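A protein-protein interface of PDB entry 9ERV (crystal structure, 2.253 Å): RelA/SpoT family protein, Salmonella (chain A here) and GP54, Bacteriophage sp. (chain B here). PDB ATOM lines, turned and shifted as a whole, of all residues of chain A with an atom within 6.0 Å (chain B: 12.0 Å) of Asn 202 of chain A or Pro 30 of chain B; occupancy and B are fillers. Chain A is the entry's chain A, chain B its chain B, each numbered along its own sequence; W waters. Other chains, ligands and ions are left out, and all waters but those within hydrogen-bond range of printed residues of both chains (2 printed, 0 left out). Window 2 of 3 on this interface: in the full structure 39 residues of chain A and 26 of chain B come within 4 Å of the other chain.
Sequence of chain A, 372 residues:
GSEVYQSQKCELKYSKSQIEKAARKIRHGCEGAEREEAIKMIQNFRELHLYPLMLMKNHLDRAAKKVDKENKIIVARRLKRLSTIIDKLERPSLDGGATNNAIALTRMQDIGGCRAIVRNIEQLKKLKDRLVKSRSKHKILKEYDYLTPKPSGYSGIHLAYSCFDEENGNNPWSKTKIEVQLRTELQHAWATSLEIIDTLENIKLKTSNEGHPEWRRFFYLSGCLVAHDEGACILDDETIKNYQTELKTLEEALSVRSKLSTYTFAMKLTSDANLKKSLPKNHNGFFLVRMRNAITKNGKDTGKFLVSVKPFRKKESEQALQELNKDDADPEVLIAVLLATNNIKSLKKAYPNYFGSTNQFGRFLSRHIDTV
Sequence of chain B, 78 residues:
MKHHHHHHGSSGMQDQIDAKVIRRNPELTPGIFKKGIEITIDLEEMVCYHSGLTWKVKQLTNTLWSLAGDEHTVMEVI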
ATOM      1  N   ILE A 197     -21.717   0.975  25.175  1.00  0.00           N
ATOM      2  CA  ILE A 197     -21.265   0.351  23.939  1.00  0.00           C
ATOM      3  C   ILE A 197     -20.985   1.396  22.842  1.00  0.00           C
ATOM      4  O   ILE A 197     -19.966   1.320  22.162  1.00  0.00           O
ATOM      5  CB  ILE A 197     -22.309  -0.692  23.458  1.00  0.00           C
ATOM      6  CG1 ILE A 197     -22.387  -1.889  24.424  1.00  0.00           C
ATOM      7  CG2 ILE A 197     -22.032  -1.146  22.008  1.00  0.00           C
ATOM      8  CD1 ILE A 197     -21.108  -2.674  24.538  1.00  0.00           C
ATOM      9  N   ASP A 198     -21.903   2.329  22.641  1.00  0.00           N
ATOM     10  CA  ASP A 198     -21.771   3.342  21.603  1.00  0.00           C
ATOM     11  C   ASP A 198     -20.547   4.217  21.806  1.00  0.00           C
ATOM     12  O   ASP A 198     -19.871   4.559  20.837  1.00  0.00           O
ATOM     13  CB  ASP A 198     -23.034   4.217  21.557  1.00  0.00           C
ATOM     14  CG  ASP A 198     -23.093   5.104  20.347  1.00  0.00           C
ATOM     15  OD1 ASP A 198     -23.189   4.571  19.238  1.00  0.00           O
ATOM     16  OD2 ASP A 198     -23.023   6.346  20.510  1.00  0.00           O
ATOM     17  N   THR A 199     -20.271   4.595  23.048  1.00  0.00           N
ATOM     18  CA  THR A 199     -19.113   5.410  23.365  1.00  0.00           C
ATOM     19  C   THR A 199     -17.809   4.601  23.251  1.00  0.00           C
ATOM     20  O   THR A 199     -16.983   4.911  22.407  1.00  0.00           O
ATOM     21  CB  THR A 199     -19.299   6.093  24.727  1.00  0.00           C
ATOM     22  OG1 THR A 199     -20.396   7.008  24.648  1.00  0.00           O
ATOM     23  CG2 THR A 199     -18.043   6.803  25.205  1.00  0.00           C
ATOM     24  N   LEU A 200     -17.659   3.535  24.047  1.00  0.00           N
ATOM     25  CA  LEU A 200     -16.447   2.738  24.103  1.00  0.00           C
ATOM     26  C   LEU A 200     -16.134   1.948  22.819  1.00  0.00           C
ATOM     27  O   LEU A 200     -14.964   1.715  22.542  1.00  0.00           O
ATOM     28  CB  LEU A 200     -16.472   1.830  25.339  1.00  0.00           C
ATOM     29  CG  LEU A 200     -16.675   2.562  26.668  1.00  0.00           C
ATOM     30  CD1 LEU A 200     -16.699   1.584  27.821  1.00  0.00           C
ATOM     31  CD2 LEU A 200     -15.598   3.635  26.898  1.00  0.00           C
ATOM     32  N   GLU A 201     -17.144   1.547  22.043  1.00  0.00           N
ATOM     33  CA  GLU A 201     -16.903   0.858  20.771  1.00  0.00           C
ATOM     34  C   GLU A 201     -16.752   1.834  19.587  1.00  0.00           C
ATOM     35  O   GLU A 201     -16.485   1.386  18.477  1.00  0.00           O
ATOM     36  CB  GLU A 201     -17.999  -0.174  20.461  1.00  0.00           C
ATOM     37  CG  GLU A 201     -18.024  -1.366  21.398  1.00  0.00           C
ATOM     38  CD  GLU A 201     -17.157  -2.519  20.948  1.00  0.00           C
ATOM     39  OE1 GLU A 201     -17.588  -3.270  20.044  1.00  0.00           O
ATOM     40  OE2 GLU A 201     -16.041  -2.670  21.494  1.00  0.00           O
ATOM     41  N   ASN A 202     -16.965   3.143  19.808  1.00  0.00           N
ATOM     42  CA  ASN A 202     -16.864   4.195  18.800  1.00  0.00           C
ATOM     43  C   ASN A 202     -17.796   3.997  17.603  1.00  0.00           C
ATOM     44  O   ASN A 202     -17.514   4.502  16.518  1.00  0.00           O
ATOM     45  CB  ASN A 202     -15.418   4.402  18.340  1.00  0.00           C
ATOM     46  CG  ASN A 202     -15.137   5.795  17.830  1.00  0.00           C
ATOM     47  OD1 ASN A 202     -16.039   6.627  17.682  1.00  0.00           O
ATOM     48  ND2 ASN A 202     -13.876   6.080  17.543  1.00  0.00           N
ATOM     49  N   ILE A 203     -18.898   3.270  17.792  1.00  0.00           N
ATOM     50  CA  ILE A 203     -19.863   3.079  16.726  1.00  0.00           C
ATOM     51  C   ILE A 203     -20.777   4.289  16.816  1.00  0.00           C
ATOM     52  O   ILE A 203     -21.354   4.534  17.873  1.00  0.00           O
ATOM     53  CB  ILE A 203     -20.574   1.708  16.843  1.00  0.00           C
ATOM     54  CG1 ILE A 203     -21.072   1.437  18.270  1.00  0.00           C
ATOM     55  CG2 ILE A 203     -19.617   0.600  16.397  1.00  0.00           C
ATOM     56  CD1 ILE A 203     -21.916   0.265  18.412  1.00  0.00           C
ATOM     57  N   LYS A 204     -20.808   5.128  15.783  1.00  0.00           N
ATOM     58  CA  LYS A 204     -21.621   6.347  15.834  1.00  0.00           C
ATOM     59  C   LYS A 204     -23.076   6.050  15.481  1.00  0.00           C
ATOM     60  O   LYS A 204     -23.511   6.365  14.377  1.00  0.00           O
ATOM     61  CB  LYS A 204     -21.015   7.443  14.947  1.00  0.00           C
ATOM     62  CG  LYS A 204     -19.734   8.044  15.532  1.00  0.00           C
ATOM     63  CD  LYS A 204     -19.171   9.151  14.637  1.00  0.00           C
ATOM     64  CE  LYS A 204     -18.975  10.457  15.376  1.00  0.00           C
ATOM     65  NZ  LYS A 204     -18.728  11.594  14.441  1.00  0.00           N
ATOM     66  N   HIS A 212     -23.001  -0.424  10.997  1.00  0.00           N
ATOM     67  CA  HIS A 212     -23.255  -1.311  12.134  1.00  0.00           C
ATOM     68  C   HIS A 212     -24.682  -1.878  12.187  1.00  0.00           C
ATOM     69  O   HIS A 212     -25.384  -1.674  13.174  1.00  0.00           O
ATOM     70  CB  HIS A 212     -22.877  -0.597  13.436  1.00  0.00           C
ATOM     71  CG  HIS A 212     -21.446  -0.158  13.425  1.00  0.00           C
ATOM     72  ND1 HIS A 212     -21.100   1.169  13.234  1.00  0.00           N
ATOM     73  CD2 HIS A 212     -20.316  -0.904  13.466  1.00  0.00           C
ATOM     74  CE1 HIS A 212     -19.777   1.195  13.229  1.00  0.00           C
ATOM     75  NE2 HIS A 212     -19.260  -0.029  13.370  1.00  0.00           N
ATOM     76  N   PHE A 286      -4.657   6.632  28.264  1.00  0.00           N
ATOM     77  CA  PHE A 286      -5.284   5.318  28.333  1.00  0.00           C
ATOM     78  C   PHE A 286      -5.132   4.582  29.678  1.00  0.00           C
ATOM     79  O   PHE A 286      -4.297   4.912  30.510  1.00  0.00           O
ATOM     80  CB  PHE A 286      -4.722   4.415  27.211  1.00  0.00           C
ATOM     81  CG  PHE A 286      -5.307   4.598  25.835  1.00  0.00           C
ATOM     82  CD1 PHE A 286      -6.676   4.715  25.655  1.00  0.00           C
ATOM     83  CD2 PHE A 286      -4.497   4.561  24.709  1.00  0.00           C
ATOM     84  CE1 PHE A 286      -7.219   4.848  24.384  1.00  0.00           C
ATOM     85  CE2 PHE A 286      -5.046   4.676  23.431  1.00  0.00           C
ATOM     86  CZ  PHE A 286      -6.403   4.830  23.279  1.00  0.00           C
ATOM     87  N   LEU A 338      -8.333  -1.650  26.358  1.00  0.00           N
ATOM     88  CA  LEU A 338      -7.717  -0.327  26.399  1.00  0.00           C
ATOM     89  C   LEU A 338      -8.837   0.724  26.480  1.00  0.00           C
ATOM     90  O   LEU A 338      -9.667   0.762  25.586  1.00  0.00           O
ATOM     91  CB  LEU A 338      -6.944  -0.124  25.096  1.00  0.00           C
ATOM     92  CG  LEU A 338      -5.718   0.764  25.159  1.00  0.00           C
ATOM     93  CD1 LEU A 338      -4.644   0.117  26.020  1.00  0.00           C
ATOM     94  CD2 LEU A 338      -5.156   0.971  23.765  1.00  0.00           C
ATOM     95  N   LEU A 339      -8.868   1.572  27.522  1.00  0.00           N
ATOM     96  CA  LEU A 339      -9.928   2.573  27.666  1.00  0.00           C
ATOM     97  C   LEU A 339      -9.397   3.970  27.912  1.00  0.00           C
ATOM     98  O   LEU A 339      -8.589   4.163  28.807  1.00  0.00           O
ATOM     99  CB  LEU A 339     -10.878   2.190  28.815  1.00  0.00           C
ATOM    100  CG  LEU A 339     -11.818   1.006  28.544  1.00  0.00           C
ATOM    101  CD1 LEU A 339     -12.628   0.664  29.776  1.00  0.00           C
ATOM    102  CD2 LEU A 339     -12.738   1.292  27.363  1.00  0.00           C
ATOM    103  N   ALA A 340      -9.898   4.954  27.172  1.00  0.00           N
ATOM    104  CA  ALA A 340      -9.500   6.344  27.356  1.00  0.00           C
ATOM    105  C   ALA A 340     -10.127   6.872  28.640  1.00  0.00           C
ATOM    106  O   ALA A 340     -11.326   6.699  28.850  1.00  0.00           O
ATOM    107  CB  ALA A 340      -9.958   7.168  26.172  1.00  0.00           C
ATOM    108  N   ASN A 343     -13.372   9.267  28.537  1.00  0.00           N
ATOM    109  CA  ASN A 343     -14.624   8.590  28.247  1.00  0.00           C
ATOM    110  C   ASN A 343     -15.164   7.874  29.467  1.00  0.00           C
ATOM    111  O   ASN A 343     -16.355   7.964  29.727  1.00  0.00           O
ATOM    112  CB  ASN A 343     -14.467   7.675  27.048  1.00  0.00           C
ATOM    113  CG  ASN A 343     -14.202   8.500  25.822  1.00  0.00           C
ATOM    114  OD1 ASN A 343     -15.113   9.117  25.258  1.00  0.00           O
ATOM    115  ND2 ASN A 343     -12.945   8.599  25.424  1.00  0.00           N
ATOM    116  N   GLU B  27     -10.091  13.017  20.940  1.00  0.00           N
ATOM    117  CA  GLU B  27      -9.614  12.733  19.584  1.00  0.00           C
ATOM    118  C   GLU B  27      -9.178  11.259  19.422  1.00  0.00           C
ATOM    119  O   GLU B  27      -9.307  10.691  18.336  1.00  0.00           O
ATOM    120  CB  GLU B  27      -8.513  13.735  19.149  1.00  0.00           C
ATOM    121  CG  GLU B  27      -7.096  13.423  19.619  1.00  0.00           C
ATOM    122  CD  GLU B  27      -6.699  13.858  21.020  1.00  0.00           C
ATOM    123  OE1 GLU B  27      -7.545  13.777  21.940  1.00  0.00           O
ATOM    124  OE2 GLU B  27      -5.530  14.270  21.202  1.00  0.00           O
ATOM    125  N   LEU B  28      -8.792  10.636  20.535  1.00  0.00           N
ATOM    126  CA  LEU B  28      -8.315   9.230  20.472  1.00  0.00           C
ATOM    127  C   LEU B  28      -9.490   8.244  20.559  1.00  0.00           C
ATOM    128  O   LEU B  28     -10.589   8.668  20.950  1.00  0.00           O
ATOM    129  CB  LEU B  28      -7.240   8.974  21.545  1.00  0.00           C
ATOM    130  N   THR B  29      -9.254   6.985  20.181  1.00  0.00           N
ATOM    131  CA  THR B  29     -10.283   5.944  20.221  1.00  0.00           C
ATOM    132  C   THR B  29     -10.716   5.722  21.677  1.00  0.00           C
ATOM    133  O   THR B  29      -9.868   5.557  22.550  1.00  0.00           O
ATOM    134  CB  THR B  29      -9.762   4.660  19.551  1.00  0.00           C
ATOM    135  OG1 THR B  29      -9.221   4.990  18.272  1.00  0.00           O
ATOM    136  CG2 THR B  29     -10.842   3.602  19.389  1.00  0.00           C
ATOM    137  N   PRO B  30     -12.027   5.765  21.971  1.00  0.00           N
ATOM    138  CA  PRO B  30     -12.468   5.634  23.367  1.00  0.00           C
ATOM    139  C   PRO B  30     -12.197   4.265  23.994  1.00  0.00           C
ATOM    140  O   PRO B  30     -11.978   4.162  25.204  1.00  0.00           O
ATOM    141  CB  PRO B  30     -13.964   5.974  23.299  1.00  0.00           C
ATOM    142  CG  PRO B  30     -14.149   6.683  21.979  1.00  0.00           C
ATOM    143  CD  PRO B  30     -13.167   6.012  21.072  1.00  0.00           C
ATOM    144  N   GLY B  31     -12.191   3.226  23.164  1.00  0.00           N
ATOM    145  CA  GLY B  31     -11.932   1.878  23.645  1.00  0.00           C
ATOM    146  C   GLY B  31     -11.494   0.898  22.580  1.00  0.00           C
ATOM    147  O   GLY B  31     -11.942   0.970  21.433  1.00  0.00           O
ATOM    148  N   ILE B  32     -10.591  -0.011  22.947  1.00  0.00           N
ATOM    149  CA  ILE B  32     -10.140  -1.071  22.062  1.00  0.00           C
ATOM    150  C   ILE B  32     -10.301  -2.368  22.838  1.00  0.00           C
ATOM    151  O   ILE B  32      -9.621  -2.572  23.843  1.00  0.00           O
ATOM    152  CB  ILE B  32      -8.691  -0.876  21.547  1.00  0.00           C
ATOM    153  CG1 ILE B  32      -8.511   0.520  20.908  1.00  0.00           C
ATOM    154  CG2 ILE B  32      -8.330  -1.995  20.563  1.00  0.00           C
ATOM    155  CD1 ILE B  32      -7.142   0.812  20.283  1.00  0.00           C
ATOM    156  N   PHE B  33     -11.240  -3.219  22.423  1.00  0.00           N
ATOM    157  CA  PHE B  33     -11.492  -4.475  23.128  1.00  0.00           C
ATOM    158  C   PHE B  33     -10.823  -5.647  22.424  1.00  0.00           C
ATOM    159  O   PHE B  33     -11.100  -5.911  21.253  1.00  0.00           O
ATOM    160  CB  PHE B  33     -13.001  -4.714  23.256  1.00  0.00           C
ATOM    161  CG  PHE B  33     -13.409  -5.979  23.979  1.00  0.00           C
ATOM    162  CD1 PHE B  33     -13.587  -7.167  23.287  1.00  0.00           C
ATOM    163  CD2 PHE B  33     -13.703  -5.958  25.331  1.00  0.00           C
ATOM    164  CE1 PHE B  33     -14.011  -8.311  23.944  1.00  0.00           C
ATOM    165  CE2 PHE B  33     -14.121  -7.106  25.982  1.00  0.00           C
ATOM    166  CZ  PHE B  33     -14.290  -8.269  25.283  1.00  0.00           C
ATOM    167  N   LYS B  34      -9.973  -6.365  23.145  1.00  0.00           N
ATOM    168  CA  LYS B  34      -9.312  -7.538  22.593  1.00  0.00           C
ATOM    169  C   LYS B  34      -9.880  -8.809  23.217  1.00  0.00           C
ATOM    170  O   LYS B  34     -10.271  -9.716  22.492  1.00  0.00           O
ATOM    171  CB  LYS B  34      -7.777  -7.460  22.763  1.00  0.00           C
ATOM    172  CG  LYS B  34      -7.096  -6.427  21.870  1.00  0.00           C
ATOM    173  CD  LYS B  34      -7.330  -6.701  20.387  1.00  0.00           C
ATOM    174  CE  LYS B  34      -6.712  -5.647  19.504  1.00  0.00           C
ATOM    175  NZ  LYS B  34      -6.995  -5.916  18.068  1.00  0.00           N
HETATM  176  O   HOH W   1     -11.599   9.680  23.378  1.00  0.00           O
HETATM  177  O   HOH W   2     -13.128  -2.172  20.093  1.00  0.00           O
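No residue of chain B comes within 4 Å of Asp 198 of chain A. Of chain B, only Pro 30 comes within 4 Å of Thr 199 of chain A. No residue of chain B comes within 4 Å of Glu 201 of chain A. Asn 202 of chain A touches just one residue of chain B: Pro 30 (3.6 Å). Ile 203 of chain A touches none of the printed residues of chain B. No residue of chain B comes within 4 Å of Lys 204 of chain A. Of the printed residues of chain B, Phe 286 of chain A touches Thr 29. Printed residues of chain B within 4 Å of Leu 338 of chain A: Gly 31 (3.2 Å) and Ile 32 (2.9 Å). Of the printed residues of chain B, Leu 339 of chain A touches Pro 30 and Gly 31. Ala 340 of chain A touches just these residues of chain B: Thr 29 (3.97 Å) and Pro 30 (3.0 Å). Asn 343 of chain A touches just one residue of chain B: Pro 30 (3.5 Å). Of the printed residues of chain A, Pro 30 of chain B touches Thr 199, Asn 202, Leu 339, Ala 340 and Asn 343. Of the printed residues of chain A, Gly 31 of chain B touches Leu 200 (3.2 Å), Leu 338 (3.2 Å) and Leu 339 (3.8 Å). The nearest printed residue of chain B that does not touch Leu 338 of chain A is Pro 30 of chain B (4.1 Å).
CB of Pro 30 of chain B touches O of Thr 199 of chain A, 3.3 Å away. CD of Pro 30 of chain B touches ND2 of Asn 202 of chain A, 3.6 Å away. Phe 286 of chain A touches Thr 29 of chain B (CE1 to O, 3.3 Å). O of Leu 338 of chain A touches CA of Gly 31 of chain B, 3.2 Å away. CA of Leu 339 of chain A touches O of Pro 30 of chain B (3.6 Å). Leu 339 of chain A touches Gly 31 of chain B (CD2 to CA, 3.8 Å). Ala 340 of chain A touches Thr 29 of chain B (CB to O, 3.97 Å). Pro 30 of chain B touches Asn 343 of chain A.
Of the 14 printed residues of chain A, 8 touch a printed residue of chain B. Hydrophobic or aromatic side chains of chain A within 4 Å of the printed part of chain B: Phe 286, Leu 338, Leu 339 and Ala 340. Hydrophobic or aromatic side chains of chain B that line the printed part of chain A: Pro 30. Among the printed residues, 11 pairs touch across the chains. Among the printed residues, no Asp or Glu carboxylate lies within 4 Å of a Lys or Arg side-chain nitrogen of the other chain.
Water W1 bridges the side-chain amide nitrogen of Asn 343 of chain A (2.7 Å) and the backbone carbonyl oxygen of Leu 28 of chain B (2.8 Å). Water W2 bridges N of Phe 33 of chain B (3.2 Å) and OE2 of Glu 201 of chain A (3.3 Å).
The backbone NH (N) of Ala 340 of chain A is in hydrogen-bond range of the backbone carbonyl oxygen (O) of Pro 30 of chain B (3.0 Å). The backbone carbonyl oxygen (O) of Leu 200 of chain A is in hydrogen-bond range of the backbone NH (N) of Gly 31 of chain B. The backbone carbonyl oxygen of Leu 338 of chain A lies within hydrogen-bond range of the backbone NH of Ile 32 of chain B, at 2.9 Å.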
